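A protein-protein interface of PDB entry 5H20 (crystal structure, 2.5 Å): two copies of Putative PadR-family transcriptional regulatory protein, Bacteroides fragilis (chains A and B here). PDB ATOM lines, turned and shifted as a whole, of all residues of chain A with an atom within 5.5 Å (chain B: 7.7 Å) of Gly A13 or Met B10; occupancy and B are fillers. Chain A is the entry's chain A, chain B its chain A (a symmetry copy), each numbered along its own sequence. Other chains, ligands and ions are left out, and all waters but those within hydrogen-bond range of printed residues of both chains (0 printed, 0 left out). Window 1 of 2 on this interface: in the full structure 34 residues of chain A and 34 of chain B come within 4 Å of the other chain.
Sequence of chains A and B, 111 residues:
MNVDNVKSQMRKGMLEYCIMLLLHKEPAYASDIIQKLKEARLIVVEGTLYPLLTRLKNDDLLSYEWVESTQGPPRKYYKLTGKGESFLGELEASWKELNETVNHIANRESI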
ATOM      1  N   SER A   8      -5.470  25.459  -7.832  1.00  0.00           N
ATOM      2  CA  SER A   8      -5.558  25.017  -9.229  1.00  0.00           C
ATOM      3  C   SER A   8      -4.285  25.285 -10.046  1.00  0.00           C
ATOM      4  O   SER A   8      -3.802  24.377 -10.736  1.00  0.00           O
ATOM      5  CB  SER A   8      -6.765  25.650  -9.922  1.00  0.00           C
ATOM      6  OG  SER A   8      -6.908  25.152 -11.239  1.00  0.00           O
ATOM      7  N   GLN A   9      -3.753  26.513  -9.963  1.00  0.00           N
ATOM      8  CA  GLN A   9      -2.566  26.896 -10.739  1.00  0.00           C
ATOM      9  C   GLN A   9      -1.320  26.154 -10.257  1.00  0.00           C
ATOM     10  O   GLN A   9      -0.489  25.721 -11.080  1.00  0.00           O
ATOM     11  CB  GLN A   9      -2.368  28.427 -10.815  1.00  0.00           C
ATOM     12  CG  GLN A   9      -2.249  29.183  -9.497  1.00  0.00           C
ATOM     13  CD  GLN A   9      -0.817  29.549  -9.145  1.00  0.00           C
ATOM     14  OE1 GLN A   9      -0.557  30.074  -8.072  1.00  0.00           O
ATOM     15  NE2 GLN A   9       0.115  29.271 -10.050  1.00  0.00           N
ATOM     16  N   MET A  10      -1.209  25.994  -8.937  1.00  0.00           N
ATOM     17  CA  MET A  10      -0.089  25.281  -8.303  1.00  0.00           C
ATOM     18  C   MET A  10      -0.067  23.782  -8.646  1.00  0.00           C
ATOM     19  O   MET A  10       1.003  23.199  -8.806  1.00  0.00           O
ATOM     20  CB  MET A  10      -0.072  25.496  -6.775  1.00  0.00           C
ATOM     21  CG  MET A  10       0.408  26.876  -6.337  1.00  0.00           C
ATOM     22  SD  MET A  10       0.788  27.070  -4.576  1.00  0.00           S
ATOM     23  CE  MET A  10       2.337  26.182  -4.449  1.00  0.00           C
ATOM     24  N   ARG A  11      -1.250  23.177  -8.751  1.00  0.00           N
ATOM     25  CA  ARG A  11      -1.390  21.771  -9.144  1.00  0.00           C
ATOM     26  C   ARG A  11      -1.107  21.549 -10.627  1.00  0.00           C
ATOM     27  O   ARG A  11      -0.499  20.536 -10.990  1.00  0.00           O
ATOM     28  CB  ARG A  11      -2.779  21.230  -8.770  1.00  0.00           C
ATOM     29  CG  ARG A  11      -2.959  20.972  -7.289  1.00  0.00           C
ATOM     30  CD  ARG A  11      -4.421  20.753  -6.923  1.00  0.00           C
ATOM     31  NE  ARG A  11      -4.550  20.460  -5.501  1.00  0.00           N
ATOM     32  CZ  ARG A  11      -5.672  20.566  -4.785  1.00  0.00           C
ATOM     33  NH1 ARG A  11      -6.811  20.976  -5.334  1.00  0.00           N
ATOM     34  NH2 ARG A  11      -5.658  20.265  -3.495  1.00  0.00           N
ATOM     35  N   LYS A  12      -1.564  22.480 -11.474  1.00  0.00           N
ATOM     36  CA  LYS A  12      -1.190  22.508 -12.907  1.00  0.00           C
ATOM     37  C   LYS A  12       0.325  22.605 -13.048  1.00  0.00           C
ATOM     38  O   LYS A  12       0.904  21.924 -13.892  1.00  0.00           O
ATOM     39  CB  LYS A  12      -1.835  23.689 -13.657  1.00  0.00           C
ATOM     40  CG  LYS A  12      -3.332  23.570 -13.869  1.00  0.00           C
ATOM     41  CD  LYS A  12      -3.881  24.686 -14.751  1.00  0.00           C
ATOM     42  CE  LYS A  12      -5.404  24.757 -14.636  1.00  0.00           C
ATOM     43  NZ  LYS A  12      -6.016  25.676 -15.638  1.00  0.00           N
ATOM     44  N   GLY A  13       0.933  23.449 -12.209  1.00  0.00           N
ATOM     45  CA  GLY A  13       2.382  23.670 -12.165  1.00  0.00           C
ATOM     46  C   GLY A  13       3.147  22.399 -11.868  1.00  0.00           C
ATOM     47  O   GLY A  13       4.102  22.060 -12.579  1.00  0.00           O
ATOM     48  N   MET A  14       2.709  21.684 -10.834  1.00  0.00           N
ATOM     49  CA  MET A  14       3.320  20.397 -10.478  1.00  0.00           C
ATOM     50  C   MET A  14       3.286  19.400 -11.651  1.00  0.00           C
ATOM     51  O   MET A  14       4.322  18.832 -12.011  1.00  0.00           O
ATOM     52  CB  MET A  14       2.703  19.805  -9.211  1.00  0.00           C
ATOM     53  CG  MET A  14       2.906  20.631  -7.940  1.00  0.00           C
ATOM     54  SD  MET A  14       4.626  20.770  -7.398  1.00  0.00           S
ATOM     55  CE  MET A  14       4.927  19.103  -6.809  1.00  0.00           C
ATOM     56  N   LEU A  15       2.105  19.235 -12.247  1.00  0.00           N
ATOM     57  CA  LEU A  15       1.902  18.372 -13.418  1.00  0.00           C
ATOM     58  C   LEU A  15       2.723  18.845 -14.632  1.00  0.00           C
ATOM     59  O   LEU A  15       3.348  18.025 -15.303  1.00  0.00           O
ATOM     60  CB  LEU A  15       0.406  18.247 -13.748  1.00  0.00           C
ATOM     61  CG  LEU A  15      -0.472  17.397 -12.803  1.00  0.00           C
ATOM     62  CD1 LEU A  15      -1.910  17.884 -12.749  1.00  0.00           C
ATOM     63  CD2 LEU A  15      -0.441  15.929 -13.198  1.00  0.00           C
ATOM     64  N   GLU A  16       2.752  20.160 -14.878  1.00  0.00           N
ATOM     65  CA  GLU A  16       3.569  20.744 -15.962  1.00  0.00           C
ATOM     66  C   GLU A  16       5.062  20.472 -15.811  1.00  0.00           C
ATOM     67  O   GLU A  16       5.748  20.213 -16.803  1.00  0.00           O
ATOM     68  CB  GLU A  16       3.334  22.248 -16.101  1.00  0.00           C
ATOM     69  CG  GLU A  16       2.075  22.606 -16.877  1.00  0.00           C
ATOM     70  CD  GLU A  16       1.610  24.021 -16.615  1.00  0.00           C
ATOM     71  OE1 GLU A  16       2.019  24.627 -15.587  1.00  0.00           O
ATOM     72  OE2 GLU A  16       0.808  24.526 -17.423  1.00  0.00           O
ATOM     73  N   TYR A  17       5.542  20.543 -14.570  1.00  0.00           N
ATOM     74  CA  TYR A  17       6.923  20.244 -14.215  1.00  0.00           C
ATOM     75  C   TYR A  17       7.219  18.762 -14.415  1.00  0.00           C
ATOM     76  O   TYR A  17       8.296  18.404 -14.882  1.00  0.00           O
ATOM     77  CB  TYR A  17       7.197  20.666 -12.765  1.00  0.00           C
ATOM     78  CG  TYR A  17       8.541  20.263 -12.213  1.00  0.00           C
ATOM     79  CD1 TYR A  17       9.656  21.096 -12.347  1.00  0.00           C
ATOM     80  CD2 TYR A  17       8.700  19.055 -11.524  1.00  0.00           C
ATOM     81  CE1 TYR A  17      10.895  20.729 -11.824  1.00  0.00           C
ATOM     82  CE2 TYR A  17       9.932  18.683 -10.996  1.00  0.00           C
ATOM     83  CZ  TYR A  17      11.025  19.525 -11.150  1.00  0.00           C
ATOM     84  OH  TYR A  17      12.236  19.156 -10.626  1.00  0.00           O
ATOM     85  N   CYS A  18       6.253  17.925 -14.052  1.00  0.00           N
ATOM     86  CA  CYS A  18       6.337  16.479 -14.202  1.00  0.00           C
ATOM     87  C   CYS A  18       6.410  16.043 -15.677  1.00  0.00           C
ATOM     88  O   CYS A  18       7.191  15.148 -16.024  1.00  0.00           O
ATOM     89  CB  CYS A  18       5.142  15.830 -13.502  1.00  0.00           C
ATOM     90  SG  CYS A  18       5.213  14.034 -13.461  1.00  0.00           S
ATOM     91  N   MET A  20       7.523  18.018 -18.200  1.00  0.00           N
ATOM     92  CA  MET A  20       8.839  18.484 -18.660  1.00  0.00           C
ATOM     93  C   MET A  20       9.950  17.563 -18.167  1.00  0.00           C
ATOM     94  O   MET A  20      10.875  17.243 -18.931  1.00  0.00           O
ATOM     95  CB  MET A  20       9.101  19.924 -18.235  1.00  0.00           C
ATOM     96  CG  MET A  20       8.240  20.935 -18.963  1.00  0.00           C
ATOM     97  SD  MET A  20       8.747  22.625 -18.612  1.00  0.00           S
ATOM     98  CE  MET A  20       7.889  22.919 -17.064  1.00  0.00           C
ATOM     99  N   LEU A  56       1.910  24.103 -22.604  1.00  0.00           N
ATOM    100  CA  LEU A  56       3.379  24.062 -22.669  1.00  0.00           C
ATOM    101  C   LEU A  56       3.907  24.247 -24.103  1.00  0.00           C
ATOM    102  O   LEU A  56       4.919  24.939 -24.298  1.00  0.00           O
ATOM    103  CB  LEU A  56       3.941  22.779 -22.036  1.00  0.00           C
ATOM    104  CG  LEU A  56       3.816  22.525 -20.515  1.00  0.00           C
ATOM    105  CD1 LEU A  56       3.781  21.035 -20.213  1.00  0.00           C
ATOM    106  CD2 LEU A  56       4.918  23.201 -19.706  1.00  0.00           C
ATOM    107  N   PHE A  87      14.348  26.235 -18.929  1.00  0.00           N
ATOM    108  CA  PHE A  87      13.350  26.496 -17.882  1.00  0.00           C
ATOM    109  C   PHE A  87      13.258  25.337 -16.891  1.00  0.00           C
ATOM    110  O   PHE A  87      13.197  25.578 -15.696  1.00  0.00           O
ATOM    111  CB  PHE A  87      11.965  26.864 -18.450  1.00  0.00           C
ATOM    112  CG  PHE A  87      10.945  27.256 -17.391  1.00  0.00           C
ATOM    113  CD1 PHE A  87      11.216  28.275 -16.460  1.00  0.00           C
ATOM    114  CD2 PHE A  87       9.696  26.636 -17.348  1.00  0.00           C
ATOM    115  CE1 PHE A  87      10.277  28.634 -15.491  1.00  0.00           C
ATOM    116  CE2 PHE A  87       8.750  27.001 -16.385  1.00  0.00           C
ATOM    117  CZ  PHE A  87       9.041  27.999 -15.453  1.00  0.00           C
ATOM    118  N   LEU A  91      14.042  25.345 -12.725  1.00  0.00           N
ATOM    119  CA  LEU A  91      13.076  24.807 -11.754  1.00  0.00           C
ATOM    120  C   LEU A  91      13.652  23.757 -10.802  1.00  0.00           C
ATOM    121  O   LEU A  91      13.335  23.768  -9.598  1.00  0.00           O
ATOM    122  CB  LEU A  91      11.872  24.218 -12.493  1.00  0.00           C
ATOM    123  CG  LEU A  91      10.545  24.953 -12.760  1.00  0.00           C
ATOM    124  CD1 LEU A  91      10.467  26.422 -12.347  1.00  0.00           C
ATOM    125  CD2 LEU A  91      10.245  24.766 -14.236  1.00  0.00           C
ATOM    126  N   ASP B   4       6.414  32.725 -20.982  1.00  0.00           N
ATOM    127  CA  ASP B   4       5.526  33.919 -20.833  1.00  0.00           C
ATOM    128  C   ASP B   4       4.478  33.720 -19.725  1.00  0.00           C
ATOM    129  O   ASP B   4       4.739  34.071 -18.571  1.00  0.00           O
ATOM    130  CB  ASP B   4       4.874  34.291 -22.177  1.00  0.00           C
ATOM    131  N   ASN B   5       3.317  33.155 -20.073  1.00  0.00           N
ATOM    132  CA  ASN B   5       2.237  32.912 -19.116  1.00  0.00           C
ATOM    133  C   ASN B   5       2.518  31.707 -18.215  1.00  0.00           C
ATOM    134  O   ASN B   5       2.411  31.818 -16.993  1.00  0.00           O
ATOM    135  CB  ASN B   5       0.882  32.776 -19.824  1.00  0.00           C
ATOM    136  CG  ASN B   5      -0.293  33.186 -18.938  1.00  0.00           C
ATOM    137  OD1 ASN B   5      -0.529  32.605 -17.872  1.00  0.00           O
ATOM    138  ND2 ASN B   5      -1.048  34.186 -19.390  1.00  0.00           N
ATOM    139  N   VAL B   6       2.882  30.573 -18.823  1.00  0.00           N
ATOM    140  CA  VAL B   6       3.257  29.343 -18.098  1.00  0.00           C
ATOM    141  C   VAL B   6       4.458  29.563 -17.162  1.00  0.00           C
ATOM    142  O   VAL B   6       4.426  29.159 -16.000  1.00  0.00           O
ATOM    143  CB  VAL B   6       3.537  28.150 -19.053  1.00  0.00           C
ATOM    144  CG1 VAL B   6       3.839  26.877 -18.267  1.00  0.00           C
ATOM    145  CG2 VAL B   6       2.356  27.906 -19.983  1.00  0.00           C
ATOM    146  N   LYS B   7       5.505  30.210 -17.669  1.00  0.00           N
ATOM    147  CA  LYS B   7       6.687  30.534 -16.863  1.00  0.00           C
ATOM    148  C   LYS B   7       6.333  31.409 -15.648  1.00  0.00           C
ATOM    149  O   LYS B   7       6.793  31.153 -14.535  1.00  0.00           O
ATOM    150  CB  LYS B   7       7.744  31.222 -17.722  1.00  0.00           C
ATOM    151  CG  LYS B   7       8.520  30.300 -18.640  1.00  0.00           C
ATOM    152  CD  LYS B   7       9.470  31.112 -19.513  1.00  0.00           C
ATOM    153  CE  LYS B   7      10.681  30.299 -19.913  1.00  0.00           C
ATOM    154  NZ  LYS B   7      11.843  31.198 -20.193  1.00  0.00           N
ATOM    155  N   SER B   8       5.498  32.420 -15.875  1.00  0.00           N
ATOM    156  CA  SER B   8       5.041  33.329 -14.817  1.00  0.00           C
ATOM    157  C   SER B   8       4.272  32.629 -13.686  1.00  0.00           C
ATOM    158  O   SER B   8       4.574  32.865 -12.508  1.00  0.00           O
ATOM    159  CB  SER B   8       4.191  34.458 -15.403  1.00  0.00           C
ATOM    160  OG  SER B   8       3.830  35.389 -14.400  1.00  0.00           O
ATOM    161  N   GLN B   9       3.299  31.779 -14.044  1.00  0.00           N
ATOM    162  CA  GLN B   9       2.466  31.093 -13.047  1.00  0.00           C
ATOM    163  C   GLN B   9       3.276  30.073 -12.250  1.00  0.00           C
ATOM    164  O   GLN B   9       3.096  29.948 -11.022  1.00  0.00           O
ATOM    165  CB  GLN B   9       1.173  30.499 -13.652  1.00  0.00           C
ATOM    166  CG  GLN B   9       1.328  29.509 -14.800  1.00  0.00           C
ATOM    167  CD  GLN B   9       1.158  28.062 -14.367  1.00  0.00           C
ATOM    168  OE1 GLN B   9       1.348  27.151 -15.160  1.00  0.00           O
ATOM    169  NE2 GLN B   9       0.798  27.849 -13.106  1.00  0.00           N
ATOM    170  N   MET B  10       4.174  29.369 -12.943  1.00  0.00           N
ATOM    171  CA  MET B  10       5.058  28.364 -12.330  1.00  0.00           C
ATOM    172  C   MET B  10       6.067  28.980 -11.346  1.00  0.00           C
ATOM    173  O   MET B  10       6.383  28.376 -10.324  1.00  0.00           O
ATOM    174  CB  MET B  10       5.780  27.517 -13.398  1.00  0.00           C
ATOM    175  CG  MET B  10       4.895  26.484 -14.088  1.00  0.00           C
ATOM    176  SD  MET B  10       5.749  25.232 -15.082  1.00  0.00           S
ATOM    177  CE  MET B  10       6.452  24.190 -13.808  1.00  0.00           C
ATOM    178  N   ARG B  11       6.561  30.175 -11.669  1.00  0.00           N
ATOM    179  CA  ARG B  11       7.475  30.918 -10.795  1.00  0.00           C
ATOM    180  C   ARG B  11       6.768  31.504  -9.575  1.00  0.00           C
ATOM    181  O   ARG B  11       7.338  31.507  -8.479  1.00  0.00           O
ATOM    182  CB  ARG B  11       8.211  32.019 -11.575  1.00  0.00           C
ATOM    183  CG  ARG B  11       9.298  31.499 -12.492  1.00  0.00           C
ATOM    184  CD  ARG B  11       9.773  32.564 -13.472  1.00  0.00           C
ATOM    185  NE  ARG B  11      10.851  32.044 -14.303  1.00  0.00           N
ATOM    186  CZ  ARG B  11      11.249  32.558 -15.470  1.00  0.00           C
ATOM    187  NH1 ARG B  11      10.662  33.628 -15.995  1.00  0.00           N
ATOM    188  NH2 ARG B  11      12.249  31.991 -16.129  1.00  0.00           N
ATOM    189  N   LYS B  12       5.546  32.012  -9.774  1.00  0.00           N
ATOM    190  CA  LYS B  12       4.660  32.421  -8.658  1.00  0.00           C
ATOM    191  C   LYS B  12       4.414  31.239  -7.729  1.00  0.00           C
ATOM    192  O   LYS B  12       4.435  31.404  -6.510  1.00  0.00           O
ATOM    193  CB  LYS B  12       3.303  32.956  -9.154  1.00  0.00           C
ATOM    194  CG  LYS B  12       3.360  34.309  -9.838  1.00  0.00           C
ATOM    195  CD  LYS B  12       1.973  34.852 -10.161  1.00  0.00           C
ATOM    196  CE  LYS B  12       2.070  36.002 -11.162  1.00  0.00           C
ATOM    197  NZ  LYS B  12       0.775  36.718 -11.346  1.00  0.00           N
ATOM    198  N   GLY B  13       4.188  30.066  -8.329  1.00  0.00           N
ATOM    199  CA  GLY B  13       3.953  28.804  -7.618  1.00  0.00           C
ATOM    200  C   GLY B  13       5.110  28.428  -6.719  1.00  0.00           C
ATOM    201  O   GLY B  13       4.912  28.119  -5.537  1.00  0.00           O
ATOM    202  N   MET B  14       6.319  28.483  -7.273  1.00  0.00           N
ATOM    203  CA  MET B  14       7.533  28.207  -6.494  1.00  0.00           C
ATOM    204  C   MET B  14       7.652  29.131  -5.268  1.00  0.00           C
ATOM    205  O   MET B  14       7.842  28.650  -4.147  1.00  0.00           O
ATOM    206  CB  MET B  14       8.790  28.250  -7.364  1.00  0.00           C
ATOM    207  CG  MET B  14       8.856  27.193  -8.467  1.00  0.00           C
ATOM    208  SD  MET B  14       8.963  25.488  -7.872  1.00  0.00           S
ATOM    209  CE  MET B  14      10.639  25.462  -7.231  1.00  0.00           C
ATOM    210  N   LEU B  15       7.504  30.435  -5.500  1.00  0.00           N
ATOM    211  CA  LEU B  15       7.525  31.453  -4.441  1.00  0.00           C
ATOM    212  C   LEU B  15       6.384  31.254  -3.427  1.00  0.00           C
ATOM    213  O   LEU B  15       6.618  31.339  -2.221  1.00  0.00           O
ATOM    214  CB  LEU B  15       7.518  32.866  -5.047  1.00  0.00           C
ATOM    215  CG  LEU B  15       8.810  33.362  -5.734  1.00  0.00           C
ATOM    216  CD1 LEU B  15       8.530  34.347  -6.856  1.00  0.00           C
ATOM    217  CD2 LEU B  15       9.762  33.988  -4.728  1.00  0.00           C
ATOM    218  N   GLU B  16       5.176  30.950  -3.914  1.00  0.00           N
ATOM    219  CA  GLU B  16       4.021  30.655  -3.040  1.00  0.00           C
ATOM    220  C   GLU B  16       4.245  29.457  -2.123  1.00  0.00           C
ATOM    221  O   GLU B  16       3.833  29.480  -0.960  1.00  0.00           O
ATOM    222  CB  GLU B  16       2.738  30.452  -3.845  1.00  0.00           C
ATOM    223  CG  GLU B  16       2.066  31.749  -4.271  1.00  0.00           C
ATOM    224  CD  GLU B  16       1.103  31.557  -5.421  1.00  0.00           C
ATOM    225  OE1 GLU B  16       1.193  30.523  -6.139  1.00  0.00           O
ATOM    226  OE2 GLU B  16       0.267  32.455  -5.632  1.00  0.00           O
ATOM    227  N   TRP B  95       6.293  16.574  -4.304  1.00  0.00           N
ATOM    228  CA  TRP B  95       7.713  16.718  -4.676  1.00  0.00           C
ATOM    229  C   TRP B  95       8.466  15.436  -4.401  1.00  0.00           C
ATOM    230  O   TRP B  95       9.400  15.095  -5.130  1.00  0.00           O
ATOM    231  CB  TRP B  95       8.413  17.815  -3.881  1.00  0.00           C
ATOM    232  CG  TRP B  95       8.001  19.167  -4.210  1.00  0.00           C
ATOM    233  CD1 TRP B  95       7.492  20.080  -3.348  1.00  0.00           C
ATOM    234  CD2 TRP B  95       8.056  19.807  -5.489  1.00  0.00           C
ATOM    235  NE1 TRP B  95       7.218  21.252  -3.996  1.00  0.00           N
ATOM    236  CE2 TRP B  95       7.554  21.115  -5.312  1.00  0.00           C
ATOM    237  CE3 TRP B  95       8.485  19.418  -6.767  1.00  0.00           C
ATOM    238  CZ2 TRP B  95       7.473  22.037  -6.344  1.00  0.00           C
ATOM    239  CZ3 TRP B  95       8.376  20.343  -7.816  1.00  0.00           C
ATOM    240  CH2 TRP B  95       7.865  21.643  -7.593  1.00  0.00           C
ATOM    241  N   LEU B  98       7.699  13.077  -7.026  1.00  0.00           N
ATOM    242  CA  LEU B  98       8.428  13.578  -8.190  1.00  0.00           C
ATOM    243  C   LEU B  98       9.902  13.127  -8.236  1.00  0.00           C
ATOM    244  O   LEU B  98      10.649  13.513  -9.145  1.00  0.00           O
ATOM    245  CB  LEU B  98       8.301  15.106  -8.242  1.00  0.00           C
ATOM    246  CG  LEU B  98       8.055  15.903  -9.528  1.00  0.00           C
ATOM    247  CD1 LEU B  98       7.576  15.085 -10.722  1.00  0.00           C
ATOM    248  CD2 LEU B  98       7.066  17.010  -9.207  1.00  0.00           C
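The side-chain carboxylate (OE1) of Glu A16 sits close to the side-chain amide oxygen (OE1) of Gln B9, 2.6 Å away. The backbone carbonyl oxygen (O) of Gln A9 lies within hydrogen-bond range of the side-chain amide nitrogen (NE2) of Gln B9. OE1 of Gln A9 lies close to OE1 of Glu B16 (2.6 Å).
Among the printed residues, merely in contact across the chains: Met A10 with Gly B13 (3.4 Å), Met A10 with Glu B16 (3.7 Å), Gly A13 with Met B10 (3.4 Å), Met A14 with Trp B95 (3.3 Å), Met A14 with Leu B98 (3.8 Å), Glu A16 with Val B6 (3.9 Å), Glu A16 with Met B10 (3.7 Å), Tyr A17 with Met B10 (3.7 Å), Tyr A17 with Trp B95 (3.9 Å), Tyr A17 with Leu B98 (3.5 Å), Cys A18 with Leu B98 (3.8 Å), Met A20 with Met B10 (3.7 Å), Phe A87 with Lys B7 (3.7 Å), Phe A87 with Met B10 (3.7 Å), Phe A87 with Arg B11 (3.7 Å), Leu A91 with Met B10 (3.9 Å) and Leu A91 with Met B14 (3.97 Å).
Gly A13 touches one residue of chain B. Printed residues of chain B within 4 Å of Glu A16: Val B6, Gln B9 and Met B10. Printed residues of chain B within 4 Å of Met A20: Met B10. Of the printed residues of chain A, Val B6 touches Glu A16 (3.9 Å). Of the printed residues of chain A, Gln B9 touches Gln A9 (3.2 Å) and Glu A16 (2.6 Å). Met B10 touches just these residues of chain A: Gly A13 (3.4 Å), Glu A16 (3.7 Å), Tyr A17 (3.7 Å), Met A20 (3.7 Å), Phe A87 (3.7 Å) and Leu A91 (3.9 Å). Lys B12 touches none of the printed residues of chain A. Of the printed residues of chain A, Met B14 touches Leu A91 (3.97 Å). The nearest printed residue of chain B that does not touch Cys A18 is Met B10 (6.3 Å).
Of the 15 printed residues of chain A, 10 touch a printed residue of chain B. Printed residues of chain A that touch a printed residue of chain B: Gln A9, Met A10, Gly A13, Met A14, Glu A16, Tyr A17, Cys A18, Met A20, Phe A87 and Leu A91. Hydrophobic or aromatic side chains of chain A within 4 Å of the printed part of chain B: Met A10, Met A14, Tyr A17, Met A20, Phe A87 and Leu A91. Of the 15 printed residues of chain B, 10 touch a printed residue of chain A. Among the printed residues, 20 pairs touch across the chains.
Gln A9 touches its own counterpart, Gln B9. Gln A9 touches Glu B16, and with the chains exchanged Glu A16 touches Gln B9. Met A10 touches Gly B13, and with the chains exchanged Gly A13 touches Met B10. Met A10 touches Glu B16, and with the chains exchanged Glu A16 touches Met B10. Positions printed for both chains: 8, 9, 10, 11, 12, 13, 14, 15 and 16.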
